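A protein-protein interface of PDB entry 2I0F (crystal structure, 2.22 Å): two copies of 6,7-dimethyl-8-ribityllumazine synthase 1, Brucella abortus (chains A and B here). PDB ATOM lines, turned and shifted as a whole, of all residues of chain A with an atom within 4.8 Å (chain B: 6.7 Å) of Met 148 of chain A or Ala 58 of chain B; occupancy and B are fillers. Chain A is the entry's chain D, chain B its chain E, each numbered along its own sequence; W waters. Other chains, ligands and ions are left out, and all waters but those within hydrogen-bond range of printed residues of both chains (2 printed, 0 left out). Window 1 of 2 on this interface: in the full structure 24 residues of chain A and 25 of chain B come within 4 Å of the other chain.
The backbone carbonyl oxygen (O) of Val 107 of chain A lies within hydrogen-bond range of the side-chain hydroxyl (OG) of Ser 61 of chain B.
The backbone carbonyl oxygen of Ser 106 of chain A is in hydrogen-bond range of the backbone NH of Ile 111 of chain A. OG1 of Thr 59 of chain B is in hydrogen-bond range of O of Glu 55 of chain B (2.6 Å).
CG2 of Val 107 of chain A touches CB of Pro 57 of chain B (3.2 Å). N of Ala 58 of chain B touches CG2 of Val 107 of chain A, 3.5 Å away. Phe 62 of chain B touches Ile 111 of chain A. Thr 147 of chain A touches Pro 51 of chain B (CG2 to CD, 3.97 Å). CE of Met 148 of chain A touches O of Glu 55 of chain B (3.4 Å). CE of Met 148 of chain A touches CB of Ala 58 of chain B, 3.8 Å away. Met 148 of chain A touches Phe 62 of chain B. Thr 49 of chain B touches Leu 151 of chain A (O to CD1, 3.2 Å). Leu 151 of chain A touches Val 50 of chain B (CD1 to CG1, 3.4 Å). Arg 152 of chain A touches Phe 62 of chain B.
Met 148 of chain A touches just these residues of chain B: Glu 55 (3.4 Å), Ala 58 (3.8 Å), Thr 59 (3.5 Å) and Phe 62 (3.4 Å). Of chain A, only Ser 106 (3.5 Å), Val 107 (3.5 Å) and Met 148 (3.8 Å) come within 4 Å of Ala 58 of chain B. Printed residues of chain A within 4 Å of Val 50 of chain B: Leu 151 (3.4 Å). Printed residues of chain A within 4 Å of Leu 105 of chain B: Val 107. The nearest residue of chain B that does not touch Met 148 of chain A is Val 50 of chain B (4.1 Å). The nearest residue of chain A that does not touch Ala 58 of chain B is Ile 111 of chain A (4.3 Å).
Of the 15 printed residues of chain B, 10 touch a printed residue of chain A. Hydrophobic or aromatic side chains of chain B that line the printed part of chain A: Val 50, Pro 51, Pro 57, Ala 58, Phe 62 and Leu 105. Along chain B the printed residues that touch a printed residue of chain A span positions 49 to 105. Among the printed residues, no Asp or Glu carboxylate lies within 4 Å of a Lys or Arg side-chain nitrogen of the other chain.
No position is printed for both chains. Of the 15 pairs that touch across the chains among the printed residues, none has its exchanged pair printed and touching as well.
Water W2 lies within hydrogen-bond range of O of Leu 54 of chain B, N of Ala 58 of chain B and OG of Ser 106 of chain A. Water W1 lies within hydrogen-bond range of the backbone carbonyl oxygen (O) of Ile 113 of chain A and the side-chain carboxylate (OE2) of Glu 55 of chain B.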
ATOM      1  N   SER A 106      -0.076   6.850   2.309  1.00  0.00           N
ATOM      2  CA  SER A 106      -0.368   7.595   1.085  1.00  0.00           C
ATOM      3  C   SER A 106       0.702   7.426   0.024  1.00  0.00           C
ATOM      4  O   SER A 106       0.402   7.373  -1.168  1.00  0.00           O
ATOM      5  CB  SER A 106      -0.554   9.090   1.382  1.00  0.00           C
ATOM      6  OG  SER A 106       0.677   9.717   1.675  1.00  0.00           O
ATOM      7  N   VAL A 107       1.958   7.366   0.452  1.00  0.00           N
ATOM      8  CA  VAL A 107       3.045   7.196  -0.493  1.00  0.00           C
ATOM      9  C   VAL A 107       3.041   5.754  -0.990  1.00  0.00           C
ATOM     10  O   VAL A 107       3.074   5.492  -2.192  1.00  0.00           O
ATOM     11  CB  VAL A 107       4.415   7.502   0.162  1.00  0.00           C
ATOM     12  CG1 VAL A 107       5.542   7.056  -0.756  1.00  0.00           C
ATOM     13  CG2 VAL A 107       4.530   8.994   0.447  1.00  0.00           C
ATOM     14  N   ILE A 111      -2.134   6.974  -2.705  1.00  0.00           N
ATOM     15  CA  ILE A 111      -3.524   7.388  -2.572  1.00  0.00           C
ATOM     16  C   ILE A 111      -3.656   8.783  -2.008  1.00  0.00           C
ATOM     17  O   ILE A 111      -2.724   9.306  -1.378  1.00  0.00           O
ATOM     18  CB  ILE A 111      -4.340   6.443  -1.669  1.00  0.00           C
ATOM     19  CG1 ILE A 111      -3.584   6.160  -0.372  1.00  0.00           C
ATOM     20  CG2 ILE A 111      -4.659   5.177  -2.410  1.00  0.00           C
ATOM     21  CD1 ILE A 111      -4.361   5.287   0.622  1.00  0.00           C
ATOM     22  N   ALA A 112      -4.830   9.369  -2.237  1.00  0.00           N
ATOM     23  CA  ALA A 112      -5.162  10.710  -1.782  1.00  0.00           C
ATOM     24  C   ALA A 112      -5.736  10.631  -0.385  1.00  0.00           C
ATOM     25  O   ALA A 112      -6.790  10.032  -0.174  1.00  0.00           O
ATOM     26  CB  ALA A 112      -6.185  11.349  -2.733  1.00  0.00           C
ATOM     27  N   ILE A 113      -5.040  11.231   0.571  1.00  0.00           N
ATOM     28  CA  ILE A 113      -5.497  11.220   1.953  1.00  0.00           C
ATOM     29  C   ILE A 113      -5.491  12.624   2.517  1.00  0.00           C
ATOM     30  O   ILE A 113      -4.465  13.302   2.489  1.00  0.00           O
ATOM     31  CB  ILE A 113      -4.577  10.387   2.880  1.00  0.00           C
ATOM     32  CG1 ILE A 113      -4.564   8.912   2.470  1.00  0.00           C
ATOM     33  CG2 ILE A 113      -5.062  10.511   4.318  1.00  0.00           C
ATOM     34  CD1 ILE A 113      -3.683   8.036   3.399  1.00  0.00           C
ATOM     35  N   ALA A 144      -8.098  18.906   1.113  1.00  0.00           N
ATOM     36  CA  ALA A 144      -6.777  18.371   0.831  1.00  0.00           C
ATOM     37  C   ALA A 144      -6.998  17.079   0.037  1.00  0.00           C
ATOM     38  O   ALA A 144      -6.412  16.873  -1.029  1.00  0.00           O
ATOM     39  CB  ALA A 144      -6.054  18.087   2.125  1.00  0.00           C
ATOM     40  N   ALA A 145      -7.867  16.225   0.560  1.00  0.00           N
ATOM     41  CA  ALA A 145      -8.185  14.968  -0.103  1.00  0.00           C
ATOM     42  C   ALA A 145      -8.567  15.212  -1.567  1.00  0.00           C
ATOM     43  O   ALA A 145      -8.018  14.581  -2.483  1.00  0.00           O
ATOM     44  CB  ALA A 145      -9.324  14.275   0.634  1.00  0.00           C
ATOM     45  N   LEU A 146      -9.494  16.141  -1.786  1.00  0.00           N
ATOM     46  CA  LEU A 146      -9.950  16.454  -3.136  1.00  0.00           C
ATOM     47  C   LEU A 146      -8.811  16.937  -3.988  1.00  0.00           C
ATOM     48  O   LEU A 146      -8.713  16.579  -5.161  1.00  0.00           O
ATOM     49  CB  LEU A 146     -11.040  17.527  -3.105  1.00  0.00           C
ATOM     50  CG  LEU A 146     -12.365  17.061  -2.505  1.00  0.00           C
ATOM     51  CD1 LEU A 146     -13.283  18.256  -2.250  1.00  0.00           C
ATOM     52  CD2 LEU A 146     -12.999  16.065  -3.462  1.00  0.00           C
ATOM     53  N   THR A 147      -7.952  17.762  -3.399  1.00  0.00           N
ATOM     54  CA  THR A 147      -6.794  18.291  -4.111  1.00  0.00           C
ATOM     55  C   THR A 147      -5.933  17.126  -4.590  1.00  0.00           C
ATOM     56  O   THR A 147      -5.578  17.040  -5.763  1.00  0.00           O
ATOM     57  CB  THR A 147      -5.955  19.185  -3.190  1.00  0.00           C
ATOM     58  OG1 THR A 147      -6.780  20.236  -2.683  1.00  0.00           O
ATOM     59  CG2 THR A 147      -4.774  19.791  -3.945  1.00  0.00           C
ATOM     60  N   MET A 148      -5.619  16.220  -3.666  1.00  0.00           N
ATOM     61  CA  MET A 148      -4.790  15.055  -3.964  1.00  0.00           C
ATOM     62  C   MET A 148      -5.448  14.158  -5.015  1.00  0.00           C
ATOM     63  O   MET A 148      -4.785  13.651  -5.925  1.00  0.00           O
ATOM     64  CB  MET A 148      -4.522  14.276  -2.679  1.00  0.00           C
ATOM     65  CG  MET A 148      -3.730  15.065  -1.652  1.00  0.00           C
ATOM     66  SD  MET A 148      -2.195  15.756  -2.334  1.00  0.00           S
ATOM     67  CE  MET A 148      -1.120  14.305  -2.333  1.00  0.00           C
ATOM     68  N   ILE A 149      -6.756  13.964  -4.890  1.00  0.00           N
ATOM     69  CA  ILE A 149      -7.479  13.162  -5.863  1.00  0.00           C
ATOM     70  C   ILE A 149      -7.266  13.794  -7.233  1.00  0.00           C
ATOM     71  O   ILE A 149      -6.958  13.102  -8.203  1.00  0.00           O
ATOM     72  CB  ILE A 149      -8.983  13.119  -5.533  1.00  0.00           C
ATOM     73  CG1 ILE A 149      -9.192  12.268  -4.280  1.00  0.00           C
ATOM     74  CG2 ILE A 149      -9.779  12.565  -6.725  1.00  0.00           C
ATOM     75  CD1 ILE A 149     -10.622  12.223  -3.789  1.00  0.00           C
ATOM     76  N   GLY A 150      -7.423  15.115  -7.303  1.00  0.00           N
ATOM     77  CA  GLY A 150      -7.228  15.816  -8.560  1.00  0.00           C
ATOM     78  C   GLY A 150      -5.800  15.663  -9.062  1.00  0.00           C
ATOM     79  O   GLY A 150      -5.559  15.487 -10.265  1.00  0.00           O
ATOM     80  N   LEU A 151      -4.837  15.731  -8.146  1.00  0.00           N
ATOM     81  CA  LEU A 151      -3.445  15.576  -8.549  1.00  0.00           C
ATOM     82  C   LEU A 151      -3.222  14.147  -9.013  1.00  0.00           C
ATOM     83  O   LEU A 151      -2.584  13.906 -10.029  1.00  0.00           O
ATOM     84  CB  LEU A 151      -2.510  15.914  -7.387  1.00  0.00           C
ATOM     85  CG  LEU A 151      -2.221  17.410  -7.242  1.00  0.00           C
ATOM     86  CD1 LEU A 151      -1.394  17.686  -5.993  1.00  0.00           C
ATOM     87  CD2 LEU A 151      -1.485  17.885  -8.480  1.00  0.00           C
ATOM     88  N   ARG A 152      -3.774  13.206  -8.262  1.00  0.00           N
ATOM     89  CA  ARG A 152      -3.649  11.795  -8.578  1.00  0.00           C
ATOM     90  C   ARG A 152      -4.171  11.499  -9.988  1.00  0.00           C
ATOM     91  O   ARG A 152      -3.585  10.693 -10.721  1.00  0.00           O
ATOM     92  CB  ARG A 152      -4.416  10.978  -7.536  1.00  0.00           C
ATOM     93  CG  ARG A 152      -4.275   9.475  -7.660  1.00  0.00           C
ATOM     94  CD  ARG A 152      -4.596   8.804  -6.322  1.00  0.00           C
ATOM     95  NE  ARG A 152      -4.570   7.351  -6.427  1.00  0.00           N
ATOM     96  CZ  ARG A 152      -5.431   6.641  -7.148  1.00  0.00           C
ATOM     97  NH1 ARG A 152      -6.390   7.257  -7.822  1.00  0.00           N
ATOM     98  NH2 ARG A 152      -5.326   5.319  -7.206  1.00  0.00           N
ATOM     99  N   LYS A 153      -5.264  12.156 -10.368  1.00  0.00           N
ATOM    100  CA  LYS A 153      -5.831  11.954 -11.694  1.00  0.00           C
ATOM    101  C   LYS A 153      -4.965  12.641 -12.731  1.00  0.00           C
ATOM    102  O   LYS A 153      -4.596  12.037 -13.740  1.00  0.00           O
ATOM    103  CB  LYS A 153      -7.263  12.498 -11.764  1.00  0.00           C
ATOM    104  CG  LYS A 153      -8.257  11.673 -10.960  1.00  0.00           C
ATOM    105  CD  LYS A 153      -9.659  12.275 -10.960  1.00  0.00           C
ATOM    106  CE  LYS A 153     -10.622  11.378 -10.182  1.00  0.00           C
ATOM    107  NZ  LYS A 153     -11.976  11.978 -10.015  1.00  0.00           N
ATOM    108  N   THR B  49       0.862  21.963  -7.054  1.00  0.00           N
ATOM    109  CA  THR B  49       0.680  22.466  -5.710  1.00  0.00           C
ATOM    110  C   THR B  49      -0.134  21.506  -4.858  1.00  0.00           C
ATOM    111  O   THR B  49      -1.016  20.821  -5.355  1.00  0.00           O
ATOM    112  CB  THR B  49      -0.038  23.846  -5.776  1.00  0.00           C
ATOM    113  OG1 THR B  49       0.784  24.767  -6.506  1.00  0.00           O
ATOM    114  CG2 THR B  49      -0.320  24.396  -4.388  1.00  0.00           C
ATOM    115  N   VAL B  50       0.179  21.470  -3.572  1.00  0.00           N
ATOM    116  CA  VAL B  50      -0.516  20.628  -2.611  1.00  0.00           C
ATOM    117  C   VAL B  50      -0.713  21.492  -1.377  1.00  0.00           C
ATOM    118  O   VAL B  50       0.024  22.450  -1.157  1.00  0.00           O
ATOM    119  CB  VAL B  50       0.320  19.397  -2.203  1.00  0.00           C
ATOM    120  CG1 VAL B  50       0.613  18.528  -3.418  1.00  0.00           C
ATOM    121  CG2 VAL B  50       1.602  19.847  -1.533  1.00  0.00           C
ATOM    122  N   PRO B  51      -1.692  21.152  -0.540  1.00  0.00           N
ATOM    123  CA  PRO B  51      -1.953  21.934   0.668  1.00  0.00           C
ATOM    124  C   PRO B  51      -0.836  21.982   1.705  1.00  0.00           C
ATOM    125  O   PRO B  51      -0.643  23.002   2.358  1.00  0.00           O
ATOM    126  CB  PRO B  51      -3.220  21.293   1.217  1.00  0.00           C
ATOM    127  CG  PRO B  51      -3.073  19.865   0.797  1.00  0.00           C
ATOM    128  CD  PRO B  51      -2.605  20.001  -0.630  1.00  0.00           C
ATOM    129  N   LEU B  54       3.216  17.550   4.111  1.00  0.00           N
ATOM    130  CA  LEU B  54       2.907  16.135   4.230  1.00  0.00           C
ATOM    131  C   LEU B  54       2.348  15.484   2.967  1.00  0.00           C
ATOM    132  O   LEU B  54       2.396  14.261   2.840  1.00  0.00           O
ATOM    133  CB  LEU B  54       1.953  15.894   5.404  1.00  0.00           C
ATOM    134  CG  LEU B  54       2.538  16.154   6.795  1.00  0.00           C
ATOM    135  CD1 LEU B  54       1.510  15.782   7.850  1.00  0.00           C
ATOM    136  CD2 LEU B  54       3.811  15.340   6.989  1.00  0.00           C
ATOM    137  N   GLU B  55       1.815  16.274   2.039  1.00  0.00           N
ATOM    138  CA  GLU B  55       1.282  15.697   0.805  1.00  0.00           C
ATOM    139  C   GLU B  55       2.302  15.680  -0.325  1.00  0.00           C
ATOM    140  O   GLU B  55       2.001  15.226  -1.432  1.00  0.00           O
ATOM    141  CB  GLU B  55       0.037  16.451   0.319  1.00  0.00           C
ATOM    142  CG  GLU B  55      -1.203  16.260   1.173  1.00  0.00           C
ATOM    143  CD  GLU B  55      -1.161  17.073   2.451  1.00  0.00           C
ATOM    144  OE1 GLU B  55      -0.759  18.247   2.389  1.00  0.00           O
ATOM    145  OE2 GLU B  55      -1.542  16.547   3.514  1.00  0.00           O
ATOM    146  N   ILE B  56       3.511  16.166  -0.070  1.00  0.00           N
ATOM    147  CA  ILE B  56       4.495  16.166  -1.139  1.00  0.00           C
ATOM    148  C   ILE B  56       4.958  14.760  -1.486  1.00  0.00           C
ATOM    149  O   ILE B  56       5.015  14.407  -2.657  1.00  0.00           O
ATOM    150  CB  ILE B  56       5.714  17.047  -0.808  1.00  0.00           C
ATOM    151  CG1 ILE B  56       5.292  18.517  -0.763  1.00  0.00           C
ATOM    152  CG2 ILE B  56       6.774  16.884  -1.887  1.00  0.00           C
ATOM    153  CD1 ILE B  56       6.246  19.419  -0.003  1.00  0.00           C
ATOM    154  N   PRO B  57       5.263  13.923  -0.482  1.00  0.00           N
ATOM    155  CA  PRO B  57       5.716  12.561  -0.806  1.00  0.00           C
ATOM    156  C   PRO B  57       4.718  11.813  -1.695  1.00  0.00           C
ATOM    157  O   PRO B  57       5.094  11.254  -2.728  1.00  0.00           O
ATOM    158  CB  PRO B  57       5.898  11.912   0.567  1.00  0.00           C
ATOM    159  CG  PRO B  57       6.187  13.088   1.461  1.00  0.00           C
ATOM    160  CD  PRO B  57       5.218  14.129   0.975  1.00  0.00           C
ATOM    161  N   ALA B  58       3.447  11.812  -1.310  1.00  0.00           N
ATOM    162  CA  ALA B  58       2.419  11.149  -2.126  1.00  0.00           C
ATOM    163  C   ALA B  58       2.381  11.742  -3.552  1.00  0.00           C
ATOM    164  O   ALA B  58       2.341  11.011  -4.545  1.00  0.00           O
ATOM    165  CB  ALA B  58       1.061  11.302  -1.477  1.00  0.00           C
ATOM    166  N   THR B  59       2.394  13.068  -3.651  1.00  0.00           N
ATOM    167  CA  THR B  59       2.353  13.730  -4.956  1.00  0.00           C
ATOM    168  C   THR B  59       3.432  13.126  -5.862  1.00  0.00           C
ATOM    169  O   THR B  59       3.164  12.728  -6.990  1.00  0.00           O
ATOM    170  CB  THR B  59       2.588  15.258  -4.817  1.00  0.00           C
ATOM    171  OG1 THR B  59       1.630  15.800  -3.901  1.00  0.00           O
ATOM    172  CG2 THR B  59       2.446  15.951  -6.160  1.00  0.00           C
ATOM    173  N   ILE B  60       4.654  13.061  -5.353  1.00  0.00           N
ATOM    174  CA  ILE B  60       5.757  12.482  -6.105  1.00  0.00           C
ATOM    175  C   ILE B  60       5.406  11.036  -6.438  1.00  0.00           C
ATOM    176  O   ILE B  60       5.669  10.553  -7.538  1.00  0.00           O
ATOM    177  CB  ILE B  60       7.037  12.500  -5.278  1.00  0.00           C
ATOM    178  CG1 ILE B  60       7.578  13.929  -5.223  1.00  0.00           C
ATOM    179  CG2 ILE B  60       8.049  11.521  -5.864  1.00  0.00           C
ATOM    180  CD1 ILE B  60       8.597  14.166  -4.150  1.00  0.00           C
ATOM    181  N   SER B  61       4.823  10.347  -5.467  1.00  0.00           N
ATOM    182  CA  SER B  61       4.420   8.970  -5.671  1.00  0.00           C
ATOM    183  C   SER B  61       3.449   8.910  -6.858  1.00  0.00           C
ATOM    184  O   SER B  61       3.525   8.002  -7.685  1.00  0.00           O
ATOM    185  CB  SER B  61       3.748   8.439  -4.418  1.00  0.00           C
ATOM    186  OG  SER B  61       3.332   7.110  -4.622  1.00  0.00           O
ATOM    187  N   PHE B  62       2.548   9.889  -6.945  1.00  0.00           N
ATOM    188  CA  PHE B  62       1.580   9.940  -8.045  1.00  0.00           C
ATOM    189  C   PHE B  62       2.306  10.072  -9.379  1.00  0.00           C
ATOM    190  O   PHE B  62       2.016   9.354 -10.327  1.00  0.00           O
ATOM    191  CB  PHE B  62       0.647  11.141  -7.899  1.00  0.00           C
ATOM    192  CG  PHE B  62      -0.238  11.087  -6.697  1.00  0.00           C
ATOM    193  CD1 PHE B  62      -0.942  12.222  -6.292  1.00  0.00           C
ATOM    194  CD2 PHE B  62      -0.371   9.918  -5.956  1.00  0.00           C
ATOM    195  CE1 PHE B  62      -1.761  12.195  -5.162  1.00  0.00           C
ATOM    196  CE2 PHE B  62      -1.192   9.885  -4.822  1.00  0.00           C
ATOM    197  CZ  PHE B  62      -1.885  11.028  -4.428  1.00  0.00           C
ATOM    198  N   ALA B  63       3.249  11.000  -9.444  1.00  0.00           N
ATOM    199  CA  ALA B  63       3.995  11.236 -10.666  1.00  0.00           C
ATOM    200  C   ALA B  63       4.744   9.993 -11.134  1.00  0.00           C
ATOM    201  O   ALA B  63       4.774   9.695 -12.327  1.00  0.00           O
ATOM    202  CB  ALA B  63       4.960  12.381 -10.464  1.00  0.00           C
ATOM    203  N   LEU B  64       5.352   9.275 -10.198  1.00  0.00           N
ATOM    204  CA  LEU B  64       6.087   8.068 -10.546  1.00  0.00           C
ATOM    205  C   LEU B  64       5.119   7.052 -11.142  1.00  0.00           C
ATOM    206  O   LEU B  64       5.403   6.446 -12.173  1.00  0.00           O
ATOM    207  CB  LEU B  64       6.772   7.484  -9.306  1.00  0.00           C
ATOM    208  CG  LEU B  64       7.890   8.338  -8.694  1.00  0.00           C
ATOM    209  CD1 LEU B  64       8.361   7.696  -7.404  1.00  0.00           C
ATOM    210  CD2 LEU B  64       9.056   8.493  -9.681  1.00  0.00           C
ATOM    211  N   LEU B 105      11.235   7.816   0.389  1.00  0.00           N
ATOM    212  CA  LEU B 105      10.771   7.751  -0.982  1.00  0.00           C
ATOM    213  C   LEU B 105      11.948   7.793  -1.940  1.00  0.00           C
ATOM    214  O   LEU B 105      11.972   7.064  -2.939  1.00  0.00           O
ATOM    215  CB  LEU B 105       9.829   8.920  -1.269  1.00  0.00           C
ATOM    216  CG  LEU B 105       9.208   8.997  -2.661  1.00  0.00           C
ATOM    217  CD1 LEU B 105       8.438   7.698  -2.938  1.00  0.00           C
ATOM    218  CD2 LEU B 105       8.282  10.219  -2.739  1.00  0.00           C
HETATM  219  O   HOH W   1      -2.030  13.724   3.445  1.00  0.00           O
HETATM  220  O   HOH W   2       2.432  12.122   1.448  1.00  0.00           O
